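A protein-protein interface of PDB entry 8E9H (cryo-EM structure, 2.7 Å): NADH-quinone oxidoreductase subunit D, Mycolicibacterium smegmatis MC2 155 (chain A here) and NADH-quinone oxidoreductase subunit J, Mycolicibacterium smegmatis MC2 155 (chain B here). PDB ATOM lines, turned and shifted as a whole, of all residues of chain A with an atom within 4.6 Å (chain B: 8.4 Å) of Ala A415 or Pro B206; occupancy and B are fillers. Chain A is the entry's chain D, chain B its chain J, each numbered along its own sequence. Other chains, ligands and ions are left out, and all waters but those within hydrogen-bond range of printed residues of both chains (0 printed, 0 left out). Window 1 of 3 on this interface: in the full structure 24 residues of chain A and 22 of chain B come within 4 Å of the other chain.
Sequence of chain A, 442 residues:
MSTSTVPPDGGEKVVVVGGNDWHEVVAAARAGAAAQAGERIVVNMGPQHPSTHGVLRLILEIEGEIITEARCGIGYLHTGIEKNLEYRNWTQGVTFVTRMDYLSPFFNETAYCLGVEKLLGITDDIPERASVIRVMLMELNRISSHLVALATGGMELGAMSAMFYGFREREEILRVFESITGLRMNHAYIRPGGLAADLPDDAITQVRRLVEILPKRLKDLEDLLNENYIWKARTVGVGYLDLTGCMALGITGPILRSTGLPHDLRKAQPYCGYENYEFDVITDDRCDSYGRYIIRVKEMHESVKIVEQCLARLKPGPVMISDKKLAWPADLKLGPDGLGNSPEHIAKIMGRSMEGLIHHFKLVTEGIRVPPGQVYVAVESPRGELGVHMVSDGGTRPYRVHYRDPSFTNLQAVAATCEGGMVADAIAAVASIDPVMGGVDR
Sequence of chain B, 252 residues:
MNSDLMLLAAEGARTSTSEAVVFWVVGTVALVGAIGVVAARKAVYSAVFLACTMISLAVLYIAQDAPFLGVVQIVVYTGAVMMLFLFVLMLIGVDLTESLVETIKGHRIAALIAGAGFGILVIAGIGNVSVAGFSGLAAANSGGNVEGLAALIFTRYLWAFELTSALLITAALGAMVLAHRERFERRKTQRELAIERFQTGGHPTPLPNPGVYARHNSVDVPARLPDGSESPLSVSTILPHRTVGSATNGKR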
ATOM      1  N   ALA A  70      17.092 -19.672   5.623  1.00  0.00           N
ATOM      2  CA  ALA A  70      16.844 -18.239   5.631  1.00  0.00           C
ATOM      3  C   ALA A  70      15.367 -17.956   5.404  1.00  0.00           C
ATOM      4  O   ALA A  70      14.722 -18.591   4.568  1.00  0.00           O
ATOM      5  CB  ALA A  70      17.672 -17.530   4.562  1.00  0.00           C
ATOM      6  N   LEU A 411      14.487  -9.687  -3.025  1.00  0.00           N
ATOM      7  CA  LEU A 411      14.662 -10.253  -1.697  1.00  0.00           C
ATOM      8  C   LEU A 411      14.291 -11.725  -1.653  1.00  0.00           C
ATOM      9  O   LEU A 411      14.712 -12.428  -0.733  1.00  0.00           O
ATOM     10  CB  LEU A 411      13.833  -9.477  -0.678  1.00  0.00           C
ATOM     11  CG  LEU A 411      14.551  -8.281  -0.057  1.00  0.00           C
ATOM     12  CD1 LEU A 411      13.589  -7.476   0.784  1.00  0.00           C
ATOM     13  CD2 LEU A 411      15.741  -8.726   0.771  1.00  0.00           C
ATOM     14  N   GLN A 412      13.518 -12.211  -2.621  1.00  0.00           N
ATOM     15  CA  GLN A 412      13.254 -13.641  -2.688  1.00  0.00           C
ATOM     16  C   GLN A 412      14.509 -14.433  -3.010  1.00  0.00           C
ATOM     17  O   GLN A 412      14.514 -15.658  -2.856  1.00  0.00           O
ATOM     18  CB  GLN A 412      12.178 -13.928  -3.728  1.00  0.00           C
ATOM     19  CG  GLN A 412      10.825 -13.367  -3.371  1.00  0.00           C
ATOM     20  CD  GLN A 412       9.778 -13.705  -4.402  1.00  0.00           C
ATOM     21  OE1 GLN A 412       9.938 -13.412  -5.583  1.00  0.00           O
ATOM     22  NE2 GLN A 412       8.706 -14.343  -3.966  1.00  0.00           N
ATOM     23  N   ALA A 413      15.570 -13.767  -3.460  1.00  0.00           N
ATOM     24  CA  ALA A 413      16.819 -14.454  -3.754  1.00  0.00           C
ATOM     25  C   ALA A 413      17.692 -14.639  -2.524  1.00  0.00           C
ATOM     26  O   ALA A 413      18.748 -15.266  -2.633  1.00  0.00           O
ATOM     27  CB  ALA A 413      17.598 -13.686  -4.817  1.00  0.00           C
ATOM     28  N   VAL A 414      17.294 -14.102  -1.371  1.00  0.00           N
ATOM     29  CA  VAL A 414      18.128 -14.219  -0.179  1.00  0.00           C
ATOM     30  C   VAL A 414      18.237 -15.671   0.255  1.00  0.00           C
ATOM     31  O   VAL A 414      19.301 -16.124   0.685  1.00  0.00           O
ATOM     32  CB  VAL A 414      17.576 -13.342   0.955  1.00  0.00           C
ATOM     33  CG1 VAL A 414      17.622 -11.881   0.563  1.00  0.00           C
ATOM     34  CG2 VAL A 414      16.175 -13.764   1.298  1.00  0.00           C
ATOM     35  N   ALA A 415      17.141 -16.423   0.167  1.00  0.00           N
ATOM     36  CA  ALA A 415      17.195 -17.819   0.577  1.00  0.00           C
ATOM     37  C   ALA A 415      18.191 -18.593  -0.272  1.00  0.00           C
ATOM     38  O   ALA A 415      18.945 -19.424   0.244  1.00  0.00           O
ATOM     39  CB  ALA A 415      15.807 -18.445   0.488  1.00  0.00           C
ATOM     40  N   ALA A 416      18.209 -18.331  -1.578  1.00  0.00           N
ATOM     41  CA  ALA A 416      19.154 -19.014  -2.451  1.00  0.00           C
ATOM     42  C   ALA A 416      20.580 -18.538  -2.209  1.00  0.00           C
ATOM     43  O   ALA A 416      21.514 -19.346  -2.193  1.00  0.00           O
ATOM     44  CB  ALA A 416      18.763 -18.799  -3.911  1.00  0.00           C
ATOM     45  N   THR A 417      20.768 -17.234  -2.016  1.00  0.00           N
ATOM     46  CA  THR A 417      22.104 -16.657  -1.959  1.00  0.00           C
ATOM     47  C   THR A 417      22.743 -16.726  -0.580  1.00  0.00           C
ATOM     48  O   THR A 417      23.941 -16.452  -0.459  1.00  0.00           O
ATOM     49  CB  THR A 417      22.063 -15.195  -2.406  1.00  0.00           C
ATOM     50  OG1 THR A 417      21.074 -14.490  -1.649  1.00  0.00           O
ATOM     51  CG2 THR A 417      21.729 -15.099  -3.879  1.00  0.00           C
ATOM     52  N   CYS A 418      21.987 -17.078   0.456  1.00  0.00           N
ATOM     53  CA  CYS A 418      22.526 -17.130   1.807  1.00  0.00           C
ATOM     54  C   CYS A 418      22.636 -18.554   2.329  1.00  0.00           C
ATOM     55  O   CYS A 418      23.613 -18.889   3.005  1.00  0.00           O
ATOM     56  CB  CYS A 418      21.653 -16.305   2.753  1.00  0.00           C
ATOM     57  SG  CYS A 418      21.540 -14.559   2.324  1.00  0.00           S
ATOM     58  N   GLU A 419      21.653 -19.399   2.032  1.00  0.00           N
ATOM     59  CA  GLU A 419      21.672 -20.765   2.530  1.00  0.00           C
ATOM     60  C   GLU A 419      22.941 -21.467   2.074  1.00  0.00           C
ATOM     61  O   GLU A 419      23.306 -21.412   0.897  1.00  0.00           O
ATOM     62  CB  GLU A 419      20.439 -21.522   2.042  1.00  0.00           C
ATOM     63  N   GLN B 190      27.236 -23.176  -0.963  1.00  0.00           N
ATOM     64  CA  GLN B 190      26.135 -22.294  -1.325  1.00  0.00           C
ATOM     65  C   GLN B 190      25.896 -22.329  -2.826  1.00  0.00           C
ATOM     66  O   GLN B 190      24.748 -22.332  -3.282  1.00  0.00           O
ATOM     67  CB  GLN B 190      26.419 -20.867  -0.867  1.00  0.00           C
ATOM     68  CG  GLN B 190      25.267 -19.916  -1.125  1.00  0.00           C
ATOM     69  CD  GLN B 190      25.363 -19.226  -2.466  1.00  0.00           C
ATOM     70  OE1 GLN B 190      26.441 -18.817  -2.890  1.00  0.00           O
ATOM     71  NE2 GLN B 190      24.234 -19.099  -3.145  1.00  0.00           N
ATOM     72  N   LEU B 193      24.251 -25.583  -3.267  1.00  0.00           N
ATOM     73  CA  LEU B 193      22.915 -25.487  -2.695  1.00  0.00           C
ATOM     74  C   LEU B 193      22.040 -24.482  -3.411  1.00  0.00           C
ATOM     75  O   LEU B 193      20.838 -24.447  -3.139  1.00  0.00           O
ATOM     76  CB  LEU B 193      22.997 -25.105  -1.217  1.00  0.00           C
ATOM     77  CG  LEU B 193      23.133 -26.237  -0.203  1.00  0.00           C
ATOM     78  CD1 LEU B 193      23.209 -25.667   1.196  1.00  0.00           C
ATOM     79  CD2 LEU B 193      21.974 -27.208  -0.313  1.00  0.00           C
ATOM     80  N   ALA B 194      22.599 -23.668  -4.302  1.00  0.00           N
ATOM     81  CA  ALA B 194      21.847 -22.643  -5.007  1.00  0.00           C
ATOM     82  C   ALA B 194      21.407 -23.097  -6.390  1.00  0.00           C
ATOM     83  O   ALA B 194      20.902 -22.280  -7.165  1.00  0.00           O
ATOM     84  CB  ALA B 194      22.675 -21.363  -5.121  1.00  0.00           C
ATOM     85  N   PHE B 198      16.001 -26.079  -8.706  1.00  0.00           N
ATOM     86  CA  PHE B 198      16.243 -24.626  -8.578  1.00  0.00           C
ATOM     87  C   PHE B 198      16.403 -24.406  -7.076  1.00  0.00           C
ATOM     88  O   PHE B 198      15.515 -23.821  -6.457  1.00  0.00           O
ATOM     89  CB  PHE B 198      15.189 -23.706  -9.176  1.00  0.00           C
ATOM     90  CG  PHE B 198      15.411 -22.294  -8.697  1.00  0.00           C
ATOM     91  CD1 PHE B 198      16.689 -21.858  -8.393  1.00  0.00           C
ATOM     92  CD2 PHE B 198      14.355 -21.425  -8.491  1.00  0.00           C
ATOM     93  CE1 PHE B 198      16.913 -20.580  -7.910  1.00  0.00           C
ATOM     94  CE2 PHE B 198      14.582 -20.140  -8.026  1.00  0.00           C
ATOM     95  CZ  PHE B 198      15.858 -19.721  -7.734  1.00  0.00           C
ATOM     96  N   GLN B 199      17.482 -24.937  -6.509  1.00  0.00           N
ATOM     97  CA  GLN B 199      17.779 -24.737  -5.072  1.00  0.00           C
ATOM     98  C   GLN B 199      16.523 -24.408  -4.282  1.00  0.00           C
ATOM     99  O   GLN B 199      15.550 -25.165  -4.398  1.00  0.00           O
ATOM    100  CB  GLN B 199      18.749 -23.577  -4.901  1.00  0.00           C
ATOM    101  N   THR B 200      16.565 -23.341  -3.475  1.00  0.00           N
ATOM    102  CA  THR B 200      15.438 -23.070  -2.595  1.00  0.00           C
ATOM    103  C   THR B 200      14.287 -22.560  -3.448  1.00  0.00           C
ATOM    104  O   THR B 200      13.283 -23.258  -3.623  1.00  0.00           O
ATOM    105  CB  THR B 200      15.824 -22.053  -1.519  1.00  0.00           C
ATOM    106  OG1 THR B 200      17.044 -22.462  -0.891  1.00  0.00           O
ATOM    107  CG2 THR B 200      14.751 -21.972  -0.458  1.00  0.00           C
ATOM    108  N   GLY B 201      14.438 -21.358  -3.999  1.00  0.00           N
ATOM    109  CA  GLY B 201      13.716 -20.956  -5.188  1.00  0.00           C
ATOM    110  C   GLY B 201      12.318 -21.515  -5.317  1.00  0.00           C
ATOM    111  O   GLY B 201      11.484 -21.364  -4.423  1.00  0.00           O
ATOM    112  N   GLY B 202      12.071 -22.188  -6.435  1.00  0.00           N
ATOM    113  CA  GLY B 202      10.816 -22.870  -6.659  1.00  0.00           C
ATOM    114  C   GLY B 202      10.323 -23.580  -5.420  1.00  0.00           C
ATOM    115  O   GLY B 202       9.116 -23.659  -5.183  1.00  0.00           O
ATOM    116  N   HIS B 203      11.246 -24.109  -4.624  1.00  0.00           N
ATOM    117  CA  HIS B 203      10.792 -24.677  -3.365  1.00  0.00           C
ATOM    118  C   HIS B 203      10.571 -23.563  -2.344  1.00  0.00           C
ATOM    119  O   HIS B 203      11.484 -22.780  -2.077  1.00  0.00           O
ATOM    120  CB  HIS B 203      11.801 -25.683  -2.835  1.00  0.00           C
ATOM    121  CG  HIS B 203      12.202 -26.711  -3.845  1.00  0.00           C
ATOM    122  ND1 HIS B 203      13.311 -26.571  -4.650  1.00  0.00           N
ATOM    123  CD2 HIS B 203      11.630 -27.887  -4.197  1.00  0.00           C
ATOM    124  CE1 HIS B 203      13.413 -27.620  -5.445  1.00  0.00           C
ATOM    125  NE2 HIS B 203      12.405 -28.434  -5.190  1.00  0.00           N
ATOM    126  N   PRO B 204       9.374 -23.525  -1.758  1.00  0.00           N
ATOM    127  CA  PRO B 204       8.890 -22.328  -1.053  1.00  0.00           C
ATOM    128  C   PRO B 204       9.788 -21.096  -1.035  1.00  0.00           C
ATOM    129  O   PRO B 204       9.917 -20.474   0.024  1.00  0.00           O
ATOM    130  CB  PRO B 204       8.677 -22.863   0.365  1.00  0.00           C
ATOM    131  CG  PRO B 204       8.274 -24.317   0.152  1.00  0.00           C
ATOM    132  CD  PRO B 204       8.715 -24.733  -1.242  1.00  0.00           C
ATOM    133  N   THR B 205      10.371 -20.706  -2.189  1.00  0.00           N
ATOM    134  CA  THR B 205      11.245 -19.538  -2.314  1.00  0.00           C
ATOM    135  C   THR B 205      11.970 -19.362  -0.982  1.00  0.00           C
ATOM    136  O   THR B 205      12.477 -20.356  -0.451  1.00  0.00           O
ATOM    137  CB  THR B 205      10.417 -18.321  -2.723  1.00  0.00           C
ATOM    138  OG1 THR B 205       9.423 -18.059  -1.728  1.00  0.00           O
ATOM    139  CG2 THR B 205       9.721 -18.583  -4.040  1.00  0.00           C
ATOM    140  N   PRO B 206      12.050 -18.171  -0.384  1.00  0.00           N
ATOM    141  CA  PRO B 206      12.329 -18.159   1.058  1.00  0.00           C
ATOM    142  C   PRO B 206      11.107 -18.654   1.815  1.00  0.00           C
ATOM    143  O   PRO B 206       9.996 -18.163   1.604  1.00  0.00           O
ATOM    144  CB  PRO B 206      12.624 -16.685   1.352  1.00  0.00           C
ATOM    145  CG  PRO B 206      13.085 -16.142   0.080  1.00  0.00           C
ATOM    146  CD  PRO B 206      12.299 -16.845  -0.972  1.00  0.00           C
ATOM    147  N   LEU B 207      11.308 -19.638   2.678  1.00  0.00           N
ATOM    148  CA  LEU B 207      10.208 -20.199   3.447  1.00  0.00           C
ATOM    149  C   LEU B 207       9.457 -19.072   4.142  1.00  0.00           C
ATOM    150  O   LEU B 207      10.051 -18.035   4.456  1.00  0.00           O
ATOM    151  CB  LEU B 207      10.727 -21.213   4.462  1.00  0.00           C
ATOM    152  CG  LEU B 207      11.233 -22.526   3.866  1.00  0.00           C
ATOM    153  CD1 LEU B 207      12.074 -23.268   4.878  1.00  0.00           C
ATOM    154  CD2 LEU B 207      10.077 -23.394   3.414  1.00  0.00           C
ATOM    155  N   PRO B 208       8.160 -19.226   4.391  1.00  0.00           N
ATOM    156  CA  PRO B 208       7.397 -18.130   4.991  1.00  0.00           C
ATOM    157  C   PRO B 208       7.985 -17.707   6.326  1.00  0.00           C
ATOM    158  O   PRO B 208       8.467 -18.528   7.108  1.00  0.00           O
ATOM    159  CB  PRO B 208       5.994 -18.720   5.158  1.00  0.00           C
ATOM    160  CG  PRO B 208       6.186 -20.190   5.109  1.00  0.00           C
ATOM    161  CD  PRO B 208       7.330 -20.421   4.188  1.00  0.00           C
ATOM    162  N   ASN B 209       7.939 -16.405   6.579  1.00  0.00           N
ATOM    163  CA  ASN B 209       8.461 -15.848   7.808  1.00  0.00           C
ATOM    164  C   ASN B 209       7.634 -16.336   8.989  1.00  0.00           C
ATOM    165  O   ASN B 209       6.466 -16.694   8.837  1.00  0.00           O
ATOM    166  CB  ASN B 209       8.433 -14.325   7.746  1.00  0.00           C
ATOM    167  CG  ASN B 209       7.034 -13.782   7.536  1.00  0.00           C
ATOM    168  OD1 ASN B 209       6.074 -14.543   7.431  1.00  0.00           O
ATOM    169  ND2 ASN B 209       6.909 -12.465   7.475  1.00  0.00           N
ATOM    170  N   LEU B 233       5.164 -24.424   7.698  1.00  0.00           N
ATOM    171  CA  LEU B 233       6.427 -23.977   7.127  1.00  0.00           C
ATOM    172  C   LEU B 233       6.933 -22.696   7.771  1.00  0.00           C
ATOM    173  O   LEU B 233       8.129 -22.404   7.681  1.00  0.00           O
ATOM    174  CB  LEU B 233       6.273 -23.759   5.624  1.00  0.00           C
ATOM    175  CG  LEU B 233       5.925 -24.990   4.788  1.00  0.00           C
ATOM    176  CD1 LEU B 233       5.804 -24.611   3.326  1.00  0.00           C
ATOM    177  CD2 LEU B 233       6.962 -26.081   4.968  1.00  0.00           C
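NE2 of Gln B190 lies within hydrogen-bond range of O of Ala A416 (2.9 Å).
Hydrophobic or aromatic side chains of chain B that line the printed part of chain A: Ala B194 and Pro B206.
Of the 10 printed residues of chain A, 5 touch a printed residue of chain B.
Hydrophobic or aromatic side chains of chain A that line the printed part of chain B: Ala A415.
Among the printed residues, no Asp or Glu carboxylate lies within 4 Å of a Lys or Arg side-chain nitrogen of the other chain.
Ala A415 touches three residues of chain B.
Pro B206 touches two residues of chain A.
Printed residues of chain B within 4 Å of Ala A416: Gln B190 (2.9 Å) and Ala B194 (3.7 Å).
Of the printed residues of chain B, Gln A412 touches Pro B206 (3.1 Å).
Printed residues of chain B within 4 Å of Thr A417: Gln B190 (3.5 Å).
Of the printed residues of chain A, Thr B205 touches Ala A415 (3.95 Å).
Of the printed residues of chain A, Gln B190 touches Ala A416, Thr A417 and Glu A419.
Printed residues of chain A within 4 Å of Thr B200: Ala A415.
The nearest residue of chain B that does not touch Ala A415 is Leu B207 (5.1 Å).
The nearest residue of chain A that does not touch Pro B206 is Val A414 (4.1 Å).
The nearest printed residue of chain A that does not touch Ala B194 is Thr A417 (5.5 Å).
The backbone carbonyl oxygen of Thr B200 sits close to a ring nitrogen (ND1) of His B203 (3.5 Å).
OG1 of Thr A417 sits at hydrogen-bond distance from O of Ala A413, at 2.6 Å.
The side-chain hydroxyl of Thr A417 sits close to the backbone carbonyl oxygen of Val A414 (3.4 Å).
CD of Pro B206 touches O of Gln A412, 3.1 Å away.
Thr B200 touches Ala A415.
Ala A415 touches Thr B205 (CB to O, 3.95 Å).
CB of Ala A415 touches CA of Pro B206 (3.5 Å).
Ala A416 touches Ala B194 (O to CB, 3.7 Å).
Gln B190 touches Thr A417.
Glu A419 touches Gln B190 (O to CG, 3.2 Å).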
